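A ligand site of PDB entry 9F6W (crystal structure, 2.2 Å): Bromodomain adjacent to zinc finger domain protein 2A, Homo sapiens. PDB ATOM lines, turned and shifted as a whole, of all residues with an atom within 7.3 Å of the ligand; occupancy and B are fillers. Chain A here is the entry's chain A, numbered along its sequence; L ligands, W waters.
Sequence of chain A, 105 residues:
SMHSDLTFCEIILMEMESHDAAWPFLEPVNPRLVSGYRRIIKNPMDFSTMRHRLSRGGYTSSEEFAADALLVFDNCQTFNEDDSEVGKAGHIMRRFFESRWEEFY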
ATOM      1  N   ALA A  22     -17.684  16.683  12.059  1.00  0.00           N
ATOM      2  CA  ALA A  22     -16.326  17.212  12.028  1.00  0.00           C
ATOM      3  C   ALA A  22     -16.084  18.274  13.087  1.00  0.00           C
ATOM      4  O   ALA A  22     -14.926  18.658  13.290  1.00  0.00           O
ATOM      5  CB  ALA A  22     -16.022  17.807  10.660  1.00  0.00           C
ATOM      6  N   TRP A  23     -17.134  18.742  13.758  1.00  0.00           N
ATOM      7  CA  TRP A  23     -16.992  19.895  14.649  1.00  0.00           C
ATOM      8  C   TRP A  23     -15.929  19.747  15.750  1.00  0.00           C
ATOM      9  O   TRP A  23     -15.376  20.778  16.133  1.00  0.00           O
ATOM     10  CB  TRP A  23     -18.363  20.228  15.255  1.00  0.00           C
ATOM     11  CG  TRP A  23     -18.938  19.116  16.058  1.00  0.00           C
ATOM     12  CD1 TRP A  23     -19.762  18.126  15.613  1.00  0.00           C
ATOM     13  CD2 TRP A  23     -18.724  18.863  17.445  1.00  0.00           C
ATOM     14  NE1 TRP A  23     -20.084  17.279  16.643  1.00  0.00           N
ATOM     15  CE2 TRP A  23     -19.445  17.699  17.778  1.00  0.00           C
ATOM     16  CE3 TRP A  23     -17.983  19.499  18.446  1.00  0.00           C
ATOM     17  CZ2 TRP A  23     -19.460  17.165  19.074  1.00  0.00           C
ATOM     18  CZ3 TRP A  23     -17.991  18.978  19.724  1.00  0.00           C
ATOM     19  CH2 TRP A  23     -18.720  17.820  20.029  1.00  0.00           C
ATOM     20  N   PRO A  24     -15.585  18.552  16.276  1.00  0.00           N
ATOM     21  CA  PRO A  24     -14.503  18.518  17.269  1.00  0.00           C
ATOM     22  C   PRO A  24     -13.104  18.594  16.691  1.00  0.00           C
ATOM     23  O   PRO A  24     -12.140  18.596  17.467  1.00  0.00           O
ATOM     24  CB  PRO A  24     -14.668  17.123  17.918  1.00  0.00           C
ATOM     25  CG  PRO A  24     -15.962  16.613  17.465  1.00  0.00           C
ATOM     26  CD  PRO A  24     -16.182  17.215  16.115  1.00  0.00           C
ATOM     27  N   PHE A  25     -12.961  18.647  15.370  1.00  0.00           N
ATOM     28  CA  PHE A  25     -11.665  18.422  14.742  1.00  0.00           C
ATOM     29  C   PHE A  25     -11.260  19.552  13.816  1.00  0.00           C
ATOM     30  O   PHE A  25     -10.161  19.494  13.247  1.00  0.00           O
ATOM     31  CB  PHE A  25     -11.634  17.079  14.005  1.00  0.00           C
ATOM     32  CG  PHE A  25     -12.158  15.947  14.825  1.00  0.00           C
ATOM     33  CD1 PHE A  25     -11.431  15.450  15.890  1.00  0.00           C
ATOM     34  CD2 PHE A  25     -13.416  15.418  14.577  1.00  0.00           C
ATOM     35  CE1 PHE A  25     -11.912  14.434  16.671  1.00  0.00           C
ATOM     36  CE2 PHE A  25     -13.897  14.391  15.367  1.00  0.00           C
ATOM     37  CZ  PHE A  25     -13.147  13.904  16.413  1.00  0.00           C
ATOM     38  N   LEU A  26     -12.084  20.592  13.691  1.00  0.00           N
ATOM     39  CA  LEU A  26     -11.810  21.686  12.779  1.00  0.00           C
ATOM     40  C   LEU A  26     -10.741  22.645  13.295  1.00  0.00           C
ATOM     41  O   LEU A  26     -10.132  23.356  12.485  1.00  0.00           O
ATOM     42  CB  LEU A  26     -13.107  22.453  12.485  1.00  0.00           C
ATOM     43  CG  LEU A  26     -14.192  21.621  11.794  1.00  0.00           C
ATOM     44  CD1 LEU A  26     -15.456  22.448  11.526  1.00  0.00           C
ATOM     45  CD2 LEU A  26     -13.620  21.099  10.488  1.00  0.00           C
ATOM     46  N   GLU A  27     -10.496  22.677  14.593  1.00  0.00           N
ATOM     47  CA  GLU A  27      -9.482  23.528  15.191  1.00  0.00           C
ATOM     48  C   GLU A  27      -8.749  22.749  16.262  1.00  0.00           C
ATOM     49  O   GLU A  27      -9.293  21.795  16.831  1.00  0.00           O
ATOM     50  CB  GLU A  27     -10.100  24.800  15.797  1.00  0.00           C
ATOM     51  CG  GLU A  27     -10.663  25.778  14.770  1.00  0.00           C
ATOM     52  CD  GLU A  27     -11.165  27.059  15.396  1.00  0.00           C
ATOM     53  OE1 GLU A  27     -10.862  27.310  16.592  1.00  0.00           O
ATOM     54  OE2 GLU A  27     -11.853  27.830  14.700  1.00  0.00           O
ATOM     55  N   PRO A  28      -7.489  23.116  16.555  1.00  0.00           N
ATOM     56  CA  PRO A  28      -6.752  22.438  17.629  1.00  0.00           C
ATOM     57  C   PRO A  28      -7.471  22.545  18.975  1.00  0.00           C
ATOM     58  O   PRO A  28      -8.063  23.576  19.300  1.00  0.00           O
ATOM     59  CB  PRO A  28      -5.412  23.182  17.680  1.00  0.00           C
ATOM     60  CG  PRO A  28      -5.286  23.863  16.362  1.00  0.00           C
ATOM     61  CD  PRO A  28      -6.691  24.182  15.928  1.00  0.00           C
ATOM     62  N   VAL A  29      -7.421  21.459  19.750  1.00  0.00           N
ATOM     63  CA  VAL A  29      -7.806  21.542  21.154  1.00  0.00           C
ATOM     64  C   VAL A  29      -6.979  22.610  21.856  1.00  0.00           C
ATOM     65  O   VAL A  29      -5.766  22.705  21.651  1.00  0.00           O
ATOM     66  CB  VAL A  29      -7.628  20.158  21.814  1.00  0.00           C
ATOM     67  CG1 VAL A  29      -7.861  20.237  23.320  1.00  0.00           C
ATOM     68  CG2 VAL A  29      -8.576  19.137  21.166  1.00  0.00           C
ATOM     69  N   ASN A  30      -7.630  23.437  22.669  1.00  0.00           N
ATOM     70  CA  ASN A  30      -6.908  24.387  23.504  1.00  0.00           C
ATOM     71  C   ASN A  30      -6.581  23.711  24.833  1.00  0.00           C
ATOM     72  O   ASN A  30      -7.493  23.512  25.646  1.00  0.00           O
ATOM     73  CB  ASN A  30      -7.728  25.663  23.727  1.00  0.00           C
ATOM     74  CG  ASN A  30      -6.938  26.748  24.483  1.00  0.00           C
ATOM     75  OD1 ASN A  30      -5.918  26.464  25.122  1.00  0.00           O
ATOM     76  ND2 ASN A  30      -7.412  27.992  24.413  1.00  0.00           N
ATOM     77  N   LEU A  33      -7.930  24.827  28.238  1.00  0.00           N
ATOM     78  CA  LEU A  33      -9.335  24.606  28.552  1.00  0.00           C
ATOM     79  C   LEU A  33      -9.652  23.150  28.847  1.00  0.00           C
ATOM     80  O   LEU A  33     -10.763  22.847  29.288  1.00  0.00           O
ATOM     81  CB  LEU A  33     -10.208  25.100  27.399  1.00  0.00           C
ATOM     82  CG  LEU A  33      -9.890  26.516  26.922  1.00  0.00           C
ATOM     83  CD1 LEU A  33     -10.697  26.892  25.672  1.00  0.00           C
ATOM     84  CD2 LEU A  33     -10.131  27.506  28.030  1.00  0.00           C
ATOM     85  N   VAL A  34      -8.715  22.234  28.636  1.00  0.00           N
ATOM     86  CA  VAL A  34      -8.981  20.804  28.750  1.00  0.00           C
ATOM     87  C   VAL A  34      -7.969  20.222  29.714  1.00  0.00           C
ATOM     88  O   VAL A  34      -6.797  20.030  29.357  1.00  0.00           O
ATOM     89  CB  VAL A  34      -8.948  20.083  27.399  1.00  0.00           C
ATOM     90  CG1 VAL A  34      -9.289  18.623  27.589  1.00  0.00           C
ATOM     91  CG2 VAL A  34      -9.928  20.745  26.415  1.00  0.00           C
ATOM     92  N   SER A  35      -8.418  19.929  30.928  1.00  0.00           N
ATOM     93  CA  SER A  35      -7.517  19.387  31.939  1.00  0.00           C
ATOM     94  C   SER A  35      -6.955  18.042  31.498  1.00  0.00           C
ATOM     95  O   SER A  35      -7.706  17.132  31.136  1.00  0.00           O
ATOM     96  CB  SER A  35      -8.254  19.266  33.273  1.00  0.00           C
ATOM     97  OG  SER A  35      -7.410  18.742  34.275  1.00  0.00           O
ATOM     98  N   TYR A  37      -4.962  17.399  28.849  1.00  0.00           N
ATOM     99  CA  TYR A  37      -4.796  17.129  27.421  1.00  0.00           C
ATOM    100  C   TYR A  37      -3.326  17.102  27.037  1.00  0.00           C
ATOM    101  O   TYR A  37      -2.863  16.184  26.344  1.00  0.00           O
ATOM    102  CB  TYR A  37      -5.524  18.183  26.587  1.00  0.00           C
ATOM    103  CG  TYR A  37      -5.643  17.742  25.156  1.00  0.00           C
ATOM    104  CD1 TYR A  37      -6.601  16.805  24.795  1.00  0.00           C
ATOM    105  CD2 TYR A  37      -4.798  18.221  24.173  1.00  0.00           C
ATOM    106  CE1 TYR A  37      -6.727  16.366  23.508  1.00  0.00           C
ATOM    107  CE2 TYR A  37      -4.917  17.784  22.842  1.00  0.00           C
ATOM    108  CZ  TYR A  37      -5.887  16.855  22.525  1.00  0.00           C
ATOM    109  OH  TYR A  37      -6.036  16.395  21.229  1.00  0.00           O
ATOM    110  N   ILE A  41      -1.899  13.716  25.426  1.00  0.00           N
ATOM    111  CA  ILE A  41      -1.796  13.702  23.973  1.00  0.00           C
ATOM    112  C   ILE A  41      -0.450  14.310  23.585  1.00  0.00           C
ATOM    113  O   ILE A  41      -0.265  15.525  23.668  1.00  0.00           O
ATOM    114  CB  ILE A  41      -2.967  14.467  23.319  1.00  0.00           C
ATOM    115  CG1 ILE A  41      -4.287  13.758  23.649  1.00  0.00           C
ATOM    116  CG2 ILE A  41      -2.777  14.610  21.818  1.00  0.00           C
ATOM    117  CD1 ILE A  41      -4.323  12.299  23.220  1.00  0.00           C
ATOM    118  N   MET A  45      -3.356  16.782  16.696  1.00  0.00           N
ATOM    119  CA  MET A  45      -3.566  16.957  15.265  1.00  0.00           C
ATOM    120  C   MET A  45      -5.029  17.326  15.076  1.00  0.00           C
ATOM    121  O   MET A  45      -5.874  16.937  15.886  1.00  0.00           O
ATOM    122  CB  MET A  45      -3.181  15.684  14.489  1.00  0.00           C
ATOM    123  CG  MET A  45      -3.247  15.810  12.959  1.00  0.00           C
ATOM    124  SD  MET A  45      -2.331  17.222  12.267  1.00  0.00           S
ATOM    125  CE  MET A  45      -0.667  16.928  12.895  1.00  0.00           C
ATOM    126  N   ASP A  46      -5.303  18.081  14.026  1.00  0.00           N
ATOM    127  CA  ASP A  46      -6.668  18.476  13.700  1.00  0.00           C
ATOM    128  C   ASP A  46      -6.734  18.835  12.218  1.00  0.00           C
ATOM    129  O   ASP A  46      -5.708  18.937  11.543  1.00  0.00           O
ATOM    130  CB  ASP A  46      -7.127  19.633  14.569  1.00  0.00           C
ATOM    131  CG  ASP A  46      -6.424  20.920  14.219  1.00  0.00           C
ATOM    132  OD1 ASP A  46      -5.251  21.077  14.609  1.00  0.00           O
ATOM    133  OD2 ASP A  46      -7.034  21.736  13.501  1.00  0.00           O
ATOM    134  N   VAL A  72      -5.494  12.129  14.246  1.00  0.00           N
ATOM    135  CA  VAL A  72      -6.671  12.797  14.785  1.00  0.00           C
ATOM    136  C   VAL A  72      -7.554  11.798  15.545  1.00  0.00           C
ATOM    137  O   VAL A  72      -7.945  12.043  16.690  1.00  0.00           O
ATOM    138  CB  VAL A  72      -7.476  13.488  13.668  1.00  0.00           C
ATOM    139  CG1 VAL A  72      -8.738  14.076  14.240  1.00  0.00           C
ATOM    140  CG2 VAL A  72      -6.655  14.583  12.977  1.00  0.00           C
ATOM    141  N   ASN A  75      -5.766  10.107  18.683  1.00  0.00           N
ATOM    142  CA  ASN A  75      -5.874  11.048  19.807  1.00  0.00           C
ATOM    143  C   ASN A  75      -7.288  11.075  20.377  1.00  0.00           C
ATOM    144  O   ASN A  75      -7.481  11.039  21.596  1.00  0.00           O
ATOM    145  CB  ASN A  75      -5.486  12.452  19.337  1.00  0.00           C
ATOM    146  CG  ASN A  75      -4.011  12.541  19.048  1.00  0.00           C
ATOM    147  OD1 ASN A  75      -3.251  11.670  19.458  1.00  0.00           O
ATOM    148  ND2 ASN A  75      -3.593  13.587  18.344  1.00  0.00           N
ATOM    149  N   CYS A  76      -8.293  11.127  19.501  1.00  0.00           N
ATOM    150  CA  CYS A  76      -9.673  11.208  19.961  1.00  0.00           C
ATOM    151  C   CYS A  76     -10.037   9.996  20.818  1.00  0.00           C
ATOM    152  O   CYS A  76     -10.604  10.138  21.917  1.00  0.00           O
ATOM    153  CB  CYS A  76     -10.599  11.303  18.754  1.00  0.00           C
ATOM    154  SG  CYS A  76     -12.318  11.431  19.218  1.00  0.00           S
ATOM    155  N   GLN A  77      -9.704   8.788  20.357  1.00  0.00           N
ATOM    156  CA  GLN A  77     -10.023   7.603  21.141  1.00  0.00           C
ATOM    157  C   GLN A  77      -9.151   7.463  22.374  1.00  0.00           C
ATOM    158  O   GLN A  77      -9.544   6.779  23.325  1.00  0.00           O
ATOM    159  CB  GLN A  77      -9.881   6.349  20.281  1.00  0.00           C
ATOM    160  CG  GLN A  77     -10.871   6.318  19.109  1.00  0.00           C
ATOM    161  CD  GLN A  77     -10.634   5.137  18.207  1.00  0.00           C
ATOM    162  OE1 GLN A  77     -11.151   4.038  18.435  1.00  0.00           O
ATOM    163  NE2 GLN A  77      -9.810   5.343  17.176  1.00  0.00           N
ATOM    164  N   PHE A  79      -8.198  10.055  24.362  1.00  0.00           N
ATOM    165  CA  PHE A  79      -8.588  10.997  25.394  1.00  0.00           C
ATOM    166  C   PHE A  79     -10.072  10.950  25.737  1.00  0.00           C
ATOM    167  O   PHE A  79     -10.442  11.249  26.873  1.00  0.00           O
ATOM    168  CB  PHE A  79      -8.224  12.426  24.988  1.00  0.00           C
ATOM    169  CG  PHE A  79      -8.269  13.396  26.137  1.00  0.00           C
ATOM    170  CD1 PHE A  79      -7.146  13.623  26.905  1.00  0.00           C
ATOM    171  CD2 PHE A  79      -9.441  14.058  26.468  1.00  0.00           C
ATOM    172  CE1 PHE A  79      -7.183  14.506  27.976  1.00  0.00           C
ATOM    173  CE2 PHE A  79      -9.481  14.929  27.533  1.00  0.00           C
ATOM    174  CZ  PHE A  79      -8.353  15.157  28.293  1.00  0.00           C
ATOM    175  N   ASN A  80     -10.939  10.590  24.797  1.00  0.00           N
ATOM    176  CA  ASN A  80     -12.373  10.691  24.990  1.00  0.00           C
ATOM    177  C   ASN A  80     -12.998   9.308  25.096  1.00  0.00           C
ATOM    178  O   ASN A  80     -12.582   8.370  24.404  1.00  0.00           O
ATOM    179  CB  ASN A  80     -13.017  11.485  23.848  1.00  0.00           C
ATOM    180  CG  ASN A  80     -12.340  12.821  23.654  1.00  0.00           C
ATOM    181  OD1 ASN A  80     -12.659  13.781  24.331  1.00  0.00           O
ATOM    182  ND2 ASN A  80     -11.344  12.868  22.759  1.00  0.00           N
ATOM    183  N   VAL A  86     -17.676  13.908  22.010  1.00  0.00           N
ATOM    184  CA  VAL A  86     -16.544  13.992  21.093  1.00  0.00           C
ATOM    185  C   VAL A  86     -16.159  12.598  20.595  1.00  0.00           C
ATOM    186  O   VAL A  86     -15.864  12.418  19.413  1.00  0.00           O
ATOM    187  CB  VAL A  86     -15.355  14.705  21.762  1.00  0.00           C
ATOM    188  CG1 VAL A  86     -14.091  14.501  20.921  1.00  0.00           C
ATOM    189  CG2 VAL A  86     -15.667  16.195  21.940  1.00  0.00           C
ATOM    190  N   GLY A  87     -16.175  11.609  21.499  1.00  0.00           N
ATOM    191  CA  GLY A  87     -15.867  10.250  21.092  1.00  0.00           C
ATOM    192  C   GLY A  87     -16.824   9.713  20.046  1.00  0.00           C
ATOM    193  O   GLY A  87     -16.402   9.104  19.048  1.00  0.00           O
HETATM  194  C1  LIG L   1     -13.825  20.276  21.176  1.00  0.00           C
HETATM  195  C2  LIG L   1     -13.704  23.787  19.655  1.00  0.00           C
HETATM  196  C3  LIG L   1     -11.640  22.593  19.367  1.00  0.00           C
HETATM  197  C4  LIG L   1     -12.410  21.278  19.220  1.00  0.00           C
HETATM  198  C5  LIG L   1     -14.039  18.270  24.558  1.00  0.00           C
HETATM  199  C6  LIG L   1     -12.844  18.987  23.935  1.00  0.00           C
HETATM  200  C7  LIG L   1     -12.424  18.448  22.522  1.00  0.00           C
HETATM  201  C8  LIG L   1     -12.836  19.060  21.354  1.00  0.00           C
HETATM  202  C9  LIG L   1     -11.526  17.384  20.740  1.00  0.00           C
HETATM  203  C10 LIG L   1     -10.762  16.458  19.779  1.00  0.00           C
HETATM  204  C11 LIG L   1     -11.571  17.389  22.143  1.00  0.00           C
HETATM  205  C12 LIG L   1     -10.779  16.398  23.013  1.00  0.00           C
HETATM  206  C13 LIG L   1     -10.528  16.670  24.500  1.00  0.00           C
HETATM  207  C14 LIG L   1     -14.438  22.445  19.821  1.00  0.00           C
HETATM  208  N1  LIG L   1     -12.296  18.381  20.319  1.00  0.00           N
HETATM  209  N2  LIG L   1     -13.574  21.287  20.103  1.00  0.00           N
HETATM  210  N3  LIG L   1     -12.462  23.698  18.927  1.00  0.00           N
HETATM  211  O1  LIG L   1     -10.328  15.396  22.538  1.00  0.00           O
HETATM  212  O2  LIG L   1     -14.795  20.353  21.861  1.00  0.00           O
HETATM  213  O   HOH W   1      -8.174  14.474  20.949  1.00  0.00           O
HETATM  214  O   HOH W   2     -13.289  22.330  16.270  1.00  0.00           O
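The backbone carbonyl oxygen of Val 86 lies within hydrogen-bond range of the side-chain sulfur of Cys 76 (3.7 Å). ND2 of Asn 80 is in hydrogen-bond range of O of Cys 76 (3.0 Å).
The backbone carbonyl oxygen (O) of Pro 24 is in hydrogen-bond range of a nitrogen (N1) of the ligand (2.9 Å). An oxygen (O1) of the ligand sits at hydrogen-bond distance from the side-chain amide nitrogen of Asn 80 (2.7 Å).
Water W1 bridges an oxygen (O1) of the ligand (2.8 Å) and the side-chain hydroxyl of Tyr 37 (2.9 Å). Water W2 lies within hydrogen-bond range of O of Trp 23 (2.6 Å), N3 of the ligand (3.1 Å), N of Glu 27 (3.3 Å) and N of Leu 26 (3.3 Å).
Merely in contact with the ligand: Phe 25, Glu 27, Pro 28, Val 29, Val 34, Tyr 37, Phe 79 and Val 86. Hydrophobic or aromatic side chains that line the ligand: Pro 24, Phe 25, Val 29, Val 34, Tyr 37, Phe 79 and Val 86. Ten residues have an atom within 4 Å of the ligand: Pro 24, Phe 25, Glu 27, Pro 28, Val 29, Val 34, Tyr 37, Phe 79, Asn 80 and Val 86. The nearest printed residue that does not touch the ligand is Trp 23 (4.1 Å).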
